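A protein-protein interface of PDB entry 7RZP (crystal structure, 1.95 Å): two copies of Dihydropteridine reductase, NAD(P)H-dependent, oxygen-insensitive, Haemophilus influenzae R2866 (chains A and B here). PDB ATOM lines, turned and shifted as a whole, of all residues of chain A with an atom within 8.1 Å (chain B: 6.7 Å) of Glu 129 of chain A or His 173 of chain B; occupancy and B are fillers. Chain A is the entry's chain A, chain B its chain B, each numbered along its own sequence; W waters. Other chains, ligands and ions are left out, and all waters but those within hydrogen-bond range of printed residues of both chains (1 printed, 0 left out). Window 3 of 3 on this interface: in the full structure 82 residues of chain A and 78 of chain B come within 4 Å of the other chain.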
ATOM      1  N   LYS A 122       2.568  18.806 -24.261  1.00  0.00           N
ATOM      2  CA  LYS A 122       1.422  18.000 -24.673  1.00  0.00           C
ATOM      3  C   LYS A 122       1.387  16.678 -23.912  1.00  0.00           C
ATOM      4  O   LYS A 122       0.366  16.316 -23.312  1.00  0.00           O
ATOM      5  CB  LYS A 122       1.494  17.737 -26.188  1.00  0.00           C
ATOM      6  CG  LYS A 122       0.375  16.802 -26.773  1.00  0.00           C
ATOM      7  CD  LYS A 122       0.286  16.826 -28.336  1.00  0.00           C
ATOM      8  CE  LYS A 122       1.680  16.474 -28.962  1.00  0.00           C
ATOM      9  NZ  LYS A 122       1.913  16.484 -30.481  1.00  0.00           N
ATOM     10  N   TYR A 123       2.501  15.942 -23.922  1.00  0.00           N
ATOM     11  CA  TYR A 123       2.500  14.619 -23.303  1.00  0.00           C
ATOM     12  C   TYR A 123       2.183  14.716 -21.820  1.00  0.00           C
ATOM     13  O   TYR A 123       1.375  13.940 -21.295  1.00  0.00           O
ATOM     14  CB  TYR A 123       3.849  13.937 -23.502  1.00  0.00           C
ATOM     15  CG  TYR A 123       4.306  13.784 -24.939  1.00  0.00           C
ATOM     16  CD1 TYR A 123       3.394  13.684 -25.992  1.00  0.00           C
ATOM     17  CD2 TYR A 123       5.660  13.746 -25.237  1.00  0.00           C
ATOM     18  CE1 TYR A 123       3.848  13.529 -27.309  1.00  0.00           C
ATOM     19  CE2 TYR A 123       6.110  13.600 -26.523  1.00  0.00           C
ATOM     20  CZ  TYR A 123       5.206  13.500 -27.550  1.00  0.00           C
ATOM     21  OH  TYR A 123       5.678  13.376 -28.828  1.00  0.00           O
ATOM     22  N   LYS A 124       2.826  15.667 -21.131  1.00  0.00           N
ATOM     23  CA  LYS A 124       2.608  15.878 -19.703  1.00  0.00           C
ATOM     24  C   LYS A 124       1.144  16.188 -19.412  1.00  0.00           C
ATOM     25  O   LYS A 124       0.554  15.623 -18.483  1.00  0.00           O
ATOM     26  CB  LYS A 124       3.512  17.009 -19.202  1.00  0.00           C
ATOM     27  CG  LYS A 124       3.219  17.438 -17.769  1.00  0.00           C
ATOM     28  CD  LYS A 124       4.340  18.235 -17.114  1.00  0.00           C
ATOM     29  CE  LYS A 124       4.012  18.475 -15.640  1.00  0.00           C
ATOM     30  NZ  LYS A 124       4.734  19.591 -14.998  1.00  0.00           N
ATOM     31  N   ALA A 125       0.541  17.092 -20.193  1.00  0.00           N
ATOM     32  CA  ALA A 125      -0.871  17.421 -20.012  1.00  0.00           C
ATOM     33  C   ALA A 125      -1.742  16.187 -20.187  1.00  0.00           C
ATOM     34  O   ALA A 125      -2.589  15.885 -19.338  1.00  0.00           O
ATOM     35  CB  ALA A 125      -1.301  18.498 -21.007  1.00  0.00           C
ATOM     36  N   LEU A 126      -1.554  15.475 -21.302  1.00  0.00           N
ATOM     37  CA  LEU A 126      -2.304  14.253 -21.568  1.00  0.00           C
ATOM     38  C   LEU A 126      -2.179  13.275 -20.414  1.00  0.00           C
ATOM     39  O   LEU A 126      -3.186  12.817 -19.858  1.00  0.00           O
ATOM     40  CB  LEU A 126      -1.821  13.604 -22.867  1.00  0.00           C
ATOM     41  CG  LEU A 126      -2.634  12.360 -23.243  1.00  0.00           C
ATOM     42  CD1 LEU A 126      -4.072  12.735 -23.658  1.00  0.00           C
ATOM     43  CD2 LEU A 126      -1.924  11.521 -24.327  1.00  0.00           C
ATOM     44  N   GLN A 127      -0.945  12.982 -20.009  1.00  0.00           N
ATOM     45  CA  GLN A 127      -0.718  11.962 -18.989  1.00  0.00           C
ATOM     46  C   GLN A 127      -1.180  12.428 -17.615  1.00  0.00           C
ATOM     47  O   GLN A 127      -1.951  11.735 -16.939  1.00  0.00           O
ATOM     48  CB  GLN A 127       0.757  11.586 -18.960  1.00  0.00           C
ATOM     49  CG  GLN A 127       1.199  10.878 -20.237  1.00  0.00           C
ATOM     50  CD  GLN A 127       2.558  10.280 -20.097  1.00  0.00           C
ATOM     51  OE1 GLN A 127       3.365  10.755 -19.294  1.00  0.00           O
ATOM     52  NE2 GLN A 127       2.827   9.213 -20.850  1.00  0.00           N
ATOM     53  N   GLU A 128      -0.730  13.597 -17.187  1.00  0.00           N
ATOM     54  CA  GLU A 128      -0.994  14.007 -15.815  1.00  0.00           C
ATOM     55  C   GLU A 128      -2.431  14.486 -15.619  1.00  0.00           C
ATOM     56  O   GLU A 128      -3.085  14.111 -14.640  1.00  0.00           O
ATOM     57  CB  GLU A 128      -0.023  15.103 -15.391  1.00  0.00           C
ATOM     58  CG  GLU A 128      -0.276  15.618 -13.978  1.00  0.00           C
ATOM     59  CD  GLU A 128       0.768  16.635 -13.542  1.00  0.00           C
ATOM     60  OE1 GLU A 128       0.934  17.660 -14.253  1.00  0.00           O
ATOM     61  OE2 GLU A 128       1.403  16.414 -12.484  1.00  0.00           O
ATOM     62  N   GLU A 129      -2.931  15.343 -16.507  1.00  0.00           N
ATOM     63  CA  GLU A 129      -4.197  16.011 -16.231  1.00  0.00           C
ATOM     64  C   GLU A 129      -5.359  15.385 -16.988  1.00  0.00           C
ATOM     65  O   GLU A 129      -6.411  15.106 -16.401  1.00  0.00           O
ATOM     66  CB  GLU A 129      -4.113  17.500 -16.592  1.00  0.00           C
ATOM     67  CG  GLU A 129      -5.416  18.257 -16.363  1.00  0.00           C
ATOM     68  CD  GLU A 129      -5.919  18.184 -14.906  1.00  0.00           C
ATOM     69  OE1 GLU A 129      -7.158  18.270 -14.680  1.00  0.00           O
ATOM     70  OE2 GLU A 129      -5.070  18.176 -13.974  1.00  0.00           O
ATOM     71  N   ASP A 130      -5.193  15.136 -18.288  1.00  0.00           N
ATOM     72  CA  ASP A 130      -6.353  14.715 -19.074  1.00  0.00           C
ATOM     73  C   ASP A 130      -6.726  13.272 -18.779  1.00  0.00           C
ATOM     74  O   ASP A 130      -7.914  12.936 -18.620  1.00  0.00           O
ATOM     75  CB  ASP A 130      -6.078  14.873 -20.553  1.00  0.00           C
ATOM     76  CG  ASP A 130      -6.095  16.306 -20.984  1.00  0.00           C
ATOM     77  OD1 ASP A 130      -6.894  17.098 -20.425  1.00  0.00           O
ATOM     78  OD2 ASP A 130      -5.284  16.629 -21.873  1.00  0.00           O
ATOM     79  N   MET A 131      -5.719  12.409 -18.683  1.00  0.00           N
ATOM     80  CA  MET A 131      -5.962  10.977 -18.697  1.00  0.00           C
ATOM     81  C   MET A 131      -5.697  10.462 -17.253  1.00  0.00           C
ATOM     82  O   MET A 131      -6.071   9.349 -16.880  1.00  0.00           O
ATOM     83  CB  MET A 131      -5.039  10.397 -19.749  1.00  0.00           C
ATOM     84  CG  MET A 131      -5.672  10.429 -21.131  1.00  0.00           C
ATOM     85  SD  MET A 131      -4.922   9.295 -22.459  1.00  0.00           S
ATOM     86  CE  MET A 131      -6.164   7.790 -22.303  1.00  0.00           C
ATOM     87  N   LYS A 132      -5.070  11.319 -16.443  1.00  0.00           N
ATOM     88  CA  LYS A 132      -4.641  11.006 -15.075  1.00  0.00           C
ATOM     89  C   LYS A 132      -3.921   9.656 -14.989  1.00  0.00           C
ATOM     90  O   LYS A 132      -4.323   8.742 -14.265  1.00  0.00           O
ATOM     91  CB  LYS A 132      -5.832  11.089 -14.119  1.00  0.00           C
ATOM     92  CG  LYS A 132      -6.635  12.397 -14.301  1.00  0.00           C
ATOM     93  CD  LYS A 132      -7.464  12.755 -13.070  1.00  0.00           C
ATOM     94  CE  LYS A 132      -7.667  14.251 -12.934  1.00  0.00           C
ATOM     95  NZ  LYS A 132      -8.301  14.830 -14.130  1.00  0.00           N
ATOM     96  N   LEU A 133      -2.826   9.549 -15.756  1.00  0.00           N
ATOM     97  CA  LEU A 133      -2.070   8.307 -15.825  1.00  0.00           C
ATOM     98  C   LEU A 133      -0.961   8.226 -14.792  1.00  0.00           C
ATOM     99  O   LEU A 133      -0.423   7.138 -14.566  1.00  0.00           O
ATOM    100  CB  LEU A 133      -1.445   8.120 -17.213  1.00  0.00           C
ATOM    101  CG  LEU A 133      -2.437   8.175 -18.363  1.00  0.00           C
ATOM    102  CD1 LEU A 133      -1.715   8.032 -19.682  1.00  0.00           C
ATOM    103  CD2 LEU A 133      -3.535   7.123 -18.174  1.00  0.00           C
ATOM    104  N   LEU A 134      -0.574   9.346 -14.192  1.00  0.00           N
ATOM    105  CA  LEU A 134       0.611   9.353 -13.356  1.00  0.00           C
ATOM    106  C   LEU A 134       0.286   9.056 -11.893  1.00  0.00           C
ATOM    107  O   LEU A 134       1.169   9.179 -11.040  1.00  0.00           O
ATOM    108  CB  LEU A 134       1.351  10.682 -13.526  1.00  0.00           C
ATOM    109  CG  LEU A 134       1.696  10.988 -14.993  1.00  0.00           C
ATOM    110  CD1 LEU A 134       2.467  12.288 -15.157  1.00  0.00           C
ATOM    111  CD2 LEU A 134       2.416   9.821 -15.715  1.00  0.00           C
ATOM    112  N   PHE B  72     -12.456  21.553 -24.231  1.00  0.00           N
ATOM    113  CA  PHE B  72     -11.648  20.574 -23.511  1.00  0.00           C
ATOM    114  C   PHE B  72     -11.220  19.407 -24.397  1.00  0.00           C
ATOM    115  O   PHE B  72     -10.760  18.382 -23.880  1.00  0.00           O
ATOM    116  CB  PHE B  72     -12.390  20.055 -22.271  1.00  0.00           C
ATOM    117  CG  PHE B  72     -13.756  19.464 -22.554  1.00  0.00           C
ATOM    118  CD1 PHE B  72     -13.895  18.110 -22.888  1.00  0.00           C
ATOM    119  CD2 PHE B  72     -14.903  20.241 -22.439  1.00  0.00           C
ATOM    120  CE1 PHE B  72     -15.157  17.542 -23.131  1.00  0.00           C
ATOM    121  CE2 PHE B  72     -16.169  19.682 -22.685  1.00  0.00           C
ATOM    122  CZ  PHE B  72     -16.296  18.330 -23.022  1.00  0.00           C
ATOM    123  N   SER B  73     -11.344  19.522 -25.718  1.00  0.00           N
ATOM    124  CA  SER B  73     -10.949  18.420 -26.588  1.00  0.00           C
ATOM    125  C   SER B  73      -9.874  18.885 -27.569  1.00  0.00           C
ATOM    126  O   SER B  73     -10.093  18.919 -28.791  1.00  0.00           O
ATOM    127  CB  SER B  73     -12.177  17.858 -27.323  1.00  0.00           C
ATOM    128  OG  SER B  73     -13.186  17.442 -26.401  1.00  0.00           O
ATOM    129  N   TRP B  74      -8.708  19.259 -27.033  1.00  0.00           N
ATOM    130  CA  TRP B  74      -7.678  19.853 -27.872  1.00  0.00           C
ATOM    131  C   TRP B  74      -7.163  18.884 -28.926  1.00  0.00           C
ATOM    132  O   TRP B  74      -6.682  19.317 -29.985  1.00  0.00           O
ATOM    133  CB  TRP B  74      -6.511  20.353 -27.021  1.00  0.00           C
ATOM    134  CG  TRP B  74      -5.972  19.310 -26.035  1.00  0.00           C
ATOM    135  CD1 TRP B  74      -6.262  19.217 -24.681  1.00  0.00           C
ATOM    136  CD2 TRP B  74      -5.057  18.224 -26.322  1.00  0.00           C
ATOM    137  NE1 TRP B  74      -5.565  18.154 -24.118  1.00  0.00           N
ATOM    138  CE2 TRP B  74      -4.835  17.524 -25.102  1.00  0.00           C
ATOM    139  CE3 TRP B  74      -4.391  17.788 -27.482  1.00  0.00           C
ATOM    140  CZ2 TRP B  74      -3.972  16.417 -25.016  1.00  0.00           C
ATOM    141  CZ3 TRP B  74      -3.529  16.684 -27.394  1.00  0.00           C
ATOM    142  CH2 TRP B  74      -3.332  16.016 -26.167  1.00  0.00           C
ATOM    143  N   GLU B 170      -7.461  10.343 -28.114  1.00  0.00           N
ATOM    144  CA  GLU B 170      -7.399  10.423 -26.655  1.00  0.00           C
ATOM    145  C   GLU B 170      -7.231  11.843 -26.122  1.00  0.00           C
ATOM    146  O   GLU B 170      -7.309  12.034 -24.900  1.00  0.00           O
ATOM    147  CB  GLU B 170      -6.251   9.582 -26.097  1.00  0.00           C
ATOM    148  CG  GLU B 170      -6.548   8.111 -25.905  1.00  0.00           C
ATOM    149  CD  GLU B 170      -5.310   7.349 -25.474  1.00  0.00           C
ATOM    150  OE1 GLU B 170      -4.269   7.987 -25.186  1.00  0.00           O
ATOM    151  OE2 GLU B 170      -5.349   6.098 -25.453  1.00  0.00           O
ATOM    152  N   GLY B 171      -6.988  12.833 -26.987  1.00  0.00           N
ATOM    153  CA  GLY B 171      -6.634  14.171 -26.531  1.00  0.00           C
ATOM    154  C   GLY B 171      -7.781  15.023 -26.025  1.00  0.00           C
ATOM    155  O   GLY B 171      -8.201  15.983 -26.679  1.00  0.00           O
ATOM    156  N   PHE B 172      -8.297  14.690 -24.847  1.00  0.00           N
ATOM    157  CA  PHE B 172      -9.338  15.488 -24.219  1.00  0.00           C
ATOM    158  C   PHE B 172      -9.324  15.209 -22.730  1.00  0.00           C
ATOM    159  O   PHE B 172      -8.778  14.206 -22.269  1.00  0.00           O
ATOM    160  CB  PHE B 172     -10.724  15.198 -24.796  1.00  0.00           C
ATOM    161  CG  PHE B 172     -11.087  13.721 -24.796  1.00  0.00           C
ATOM    162  CD1 PHE B 172     -11.641  13.123 -23.670  1.00  0.00           C
ATOM    163  CD2 PHE B 172     -10.867  12.947 -25.937  1.00  0.00           C
ATOM    164  CE1 PHE B 172     -11.973  11.766 -23.682  1.00  0.00           C
ATOM    165  CE2 PHE B 172     -11.220  11.562 -25.966  1.00  0.00           C
ATOM    166  CZ  PHE B 172     -11.757  10.993 -24.819  1.00  0.00           C
ATOM    167  N   HIS B 173      -9.930  16.125 -21.986  1.00  0.00           N
ATOM    168  CA  HIS B 173     -10.032  15.984 -20.547  1.00  0.00           C
ATOM    169  C   HIS B 173     -11.097  14.944 -20.252  1.00  0.00           C
ATOM    170  O   HIS B 173     -12.287  15.213 -20.435  1.00  0.00           O
ATOM    171  CB  HIS B 173     -10.379  17.326 -19.916  1.00  0.00           C
ATOM    172  CG  HIS B 173     -10.040  17.395 -18.466  1.00  0.00           C
ATOM    173  ND1 HIS B 173     -10.846  16.849 -17.492  1.00  0.00           N
ATOM    174  CD2 HIS B 173      -8.968  17.918 -17.823  1.00  0.00           C
ATOM    175  CE1 HIS B 173     -10.293  17.042 -16.307  1.00  0.00           C
ATOM    176  NE2 HIS B 173      -9.153  17.692 -16.479  1.00  0.00           N
ATOM    177  N   TYR B 174     -10.673  13.756 -19.804  1.00  0.00           N
ATOM    178  CA  TYR B 174     -11.610  12.659 -19.559  1.00  0.00           C
ATOM    179  C   TYR B 174     -12.656  13.012 -18.498  1.00  0.00           C
ATOM    180  O   TYR B 174     -13.833  12.700 -18.671  1.00  0.00           O
ATOM    181  CB  TYR B 174     -10.827  11.398 -19.184  1.00  0.00           C
ATOM    182  CG  TYR B 174     -10.451  10.597 -20.404  1.00  0.00           C
ATOM    183  CD1 TYR B 174      -9.459  11.043 -21.260  1.00  0.00           C
ATOM    184  CD2 TYR B 174     -11.087   9.396 -20.699  1.00  0.00           C
ATOM    185  CE1 TYR B 174      -9.117  10.330 -22.388  1.00  0.00           C
ATOM    186  CE2 TYR B 174     -10.741   8.668 -21.829  1.00  0.00           C
ATOM    187  CZ  TYR B 174      -9.763   9.139 -22.673  1.00  0.00           C
ATOM    188  OH  TYR B 174      -9.402   8.411 -23.798  1.00  0.00           O
ATOM    189  N   ASP B 175     -12.260  13.669 -17.409  1.00  0.00           N
ATOM    190  CA  ASP B 175     -13.245  14.044 -16.386  1.00  0.00           C
ATOM    191  C   ASP B 175     -14.300  15.003 -16.938  1.00  0.00           C
ATOM    192  O   ASP B 175     -15.494  14.875 -16.623  1.00  0.00           O
ATOM    193  CB  ASP B 175     -12.566  14.665 -15.160  1.00  0.00           C
ATOM    194  CG  ASP B 175     -11.849  13.629 -14.282  1.00  0.00           C
ATOM    195  OD1 ASP B 175     -12.097  12.408 -14.423  1.00  0.00           O
ATOM    196  OD2 ASP B 175     -11.033  14.040 -13.437  1.00  0.00           O
ATOM    197  N   LYS B 176     -13.886  15.985 -17.744  1.00  0.00           N
ATOM    198  CA  LYS B 176     -14.870  16.925 -18.271  1.00  0.00           C
ATOM    199  C   LYS B 176     -15.771  16.290 -19.318  1.00  0.00           C
ATOM    200  O   LYS B 176     -16.957  16.630 -19.391  1.00  0.00           O
ATOM    201  CB  LYS B 176     -14.200  18.191 -18.802  1.00  0.00           C
ATOM    202  CG  LYS B 176     -13.891  19.026 -17.567  1.00  0.00           C
ATOM    203  CD  LYS B 176     -12.718  19.966 -17.564  1.00  0.00           C
ATOM    204  CE  LYS B 176     -13.280  21.404 -17.582  1.00  0.00           C
ATOM    205  NZ  LYS B 176     -12.411  22.480 -18.083  1.00  0.00           N
ATOM    206  N   MET B 177     -15.251  15.362 -20.100  1.00  0.00           N
ATOM    207  CA  MET B 177     -16.029  14.718 -21.150  1.00  0.00           C
ATOM    208  C   MET B 177     -17.054  13.754 -20.542  1.00  0.00           C
ATOM    209  O   MET B 177     -18.212  13.735 -20.956  1.00  0.00           O
ATOM    210  CB  MET B 177     -15.097  13.970 -22.105  1.00  0.00           C
ATOM    211  CG  MET B 177     -15.803  13.174 -23.221  1.00  0.00           C
ATOM    212  SD  MET B 177     -16.421  14.240 -24.708  1.00  0.00           S
ATOM    213  CE  MET B 177     -14.645  14.821 -25.356  1.00  0.00           C
ATOM    214  N   ASN B 178     -16.610  12.923 -19.592  1.00  0.00           N
ATOM    215  CA  ASN B 178     -17.540  12.126 -18.792  1.00  0.00           C
ATOM    216  C   ASN B 178     -18.654  13.003 -18.226  1.00  0.00           C
ATOM    217  O   ASN B 178     -19.848  12.712 -18.387  1.00  0.00           O
ATOM    218  CB  ASN B 178     -16.785  11.453 -17.644  1.00  0.00           C
ATOM    219  CG  ASN B 178     -16.167  10.106 -18.038  1.00  0.00           C
ATOM    220  OD1 ASN B 178     -16.839   9.252 -18.604  1.00  0.00           O
ATOM    221  ND2 ASN B 178     -14.892   9.893 -17.670  1.00  0.00           N
HETATM  222  O   HOH W   1      -9.400  13.814 -16.389  1.00  0.00           O
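A ring nitrogen (NE2) of His 173 of chain B sits at hydrogen-bond distance from the side-chain carboxylate (OE1) of Glu 129 of chain A (2.7 Å). The side-chain carboxylate (OD2) of Asp 130 of chain A lies within hydrogen-bond range of the indole nitrogen (NE1) of Trp 74 of chain B, at 2.7 Å. The backbone carbonyl oxygen (O) of Asp 130 of chain A is in hydrogen-bond range of the backbone NH (N) of Tyr 174 of chain B, 3.1 Å away. OD2 of Asp 175 of chain B lies within salt-bridge range of NZ of Lys 132 of chain A (2.9 Å). SD of Met 131 of chain A lies close to OE1 of Glu 170 of chain B.
The backbone NH (N) of Asp 130 of chain A sits at hydrogen-bond distance from the backbone carbonyl oxygen (O) of Ala 125 of chain A (2.9 Å). O of Leu 126 of chain A is in hydrogen-bond range of N of Met 131 of chain A, at 2.8 Å. The side-chain carboxylate of Glu 129 of chain A lies within salt-bridge range of the side-chain amino group of Lys 132 of chain A (3.7 Å). The backbone carbonyl oxygen of Phe 72 of chain B sits at hydrogen-bond distance from the backbone NH of His 173 of chain B (3.1 Å). The backbone NH of Trp 74 of chain B lies within hydrogen-bond range of the backbone carbonyl oxygen of Gly 171 of chain B. A ring nitrogen (ND1) of His 173 of chain B sits close to the backbone NH (N) of Asp 175 of chain B, 3.5 Å away.
Among the printed residues, merely in contact across the chains: Lys 122 of chain A with Trp 74 of chain B (3.8 Å), Leu 126 of chain A with Trp 74 of chain B (3.9 Å), Leu 126 of chain A with Glu 170 of chain B (3.5 Å), Asp 130 of chain A with Phe 172 of chain B (3.3 Å), Asp 130 of chain A with His 173 of chain B (3.3 Å), Met 131 of chain A with Tyr 174 of chain B (3.6 Å) and Lys 132 of chain A with His 173 of chain B (3.7 Å).
Glu 129 of chain A touches just one residue of chain B: His 173. Of the printed residues of chain A, Tyr 174 of chain B touches Asp 130 and Met 131. Printed residues of chain B within 4 Å of Lys 122 of chain A: Trp 74. Printed residues of chain A within 4 Å of Glu 170 of chain B: Leu 126 and Met 131. Printed residues of chain B within 4 Å of Lys 132 of chain A: His 173 (3.7 Å) and Asp 175 (2.9 Å). Printed residues of chain B within 4 Å of Leu 126 of chain A: Trp 74 and Glu 170. Tyr 123 of chain A touches none of the printed residues of chain B. Met 177 of chain B touches none of the printed residues of chain A.
Of the 12 printed residues of chain B, 6 touch a printed residue of chain A. Of the 13 printed residues of chain A, 6 touch a printed residue of chain B. Hydrophobic or aromatic side chains of chain A within 4 Å of the printed part of chain B: Leu 126 and Met 131. Among the printed residues, 12 pairs touch across the chains.
No position is printed for both chains. Of the 12 pairs that touch across the chains among the printed residues, none has its exchanged pair printed and touching as well.
Water W1 lies within hydrogen-bond range of the side-chain amino group of Lys 132 of chain A, the backbone carbonyl oxygen of Asp 130 of chain A, the backbone NH of Asp 175 of chain B and the backbone carbonyl oxygen of Glu 129 of chain A.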
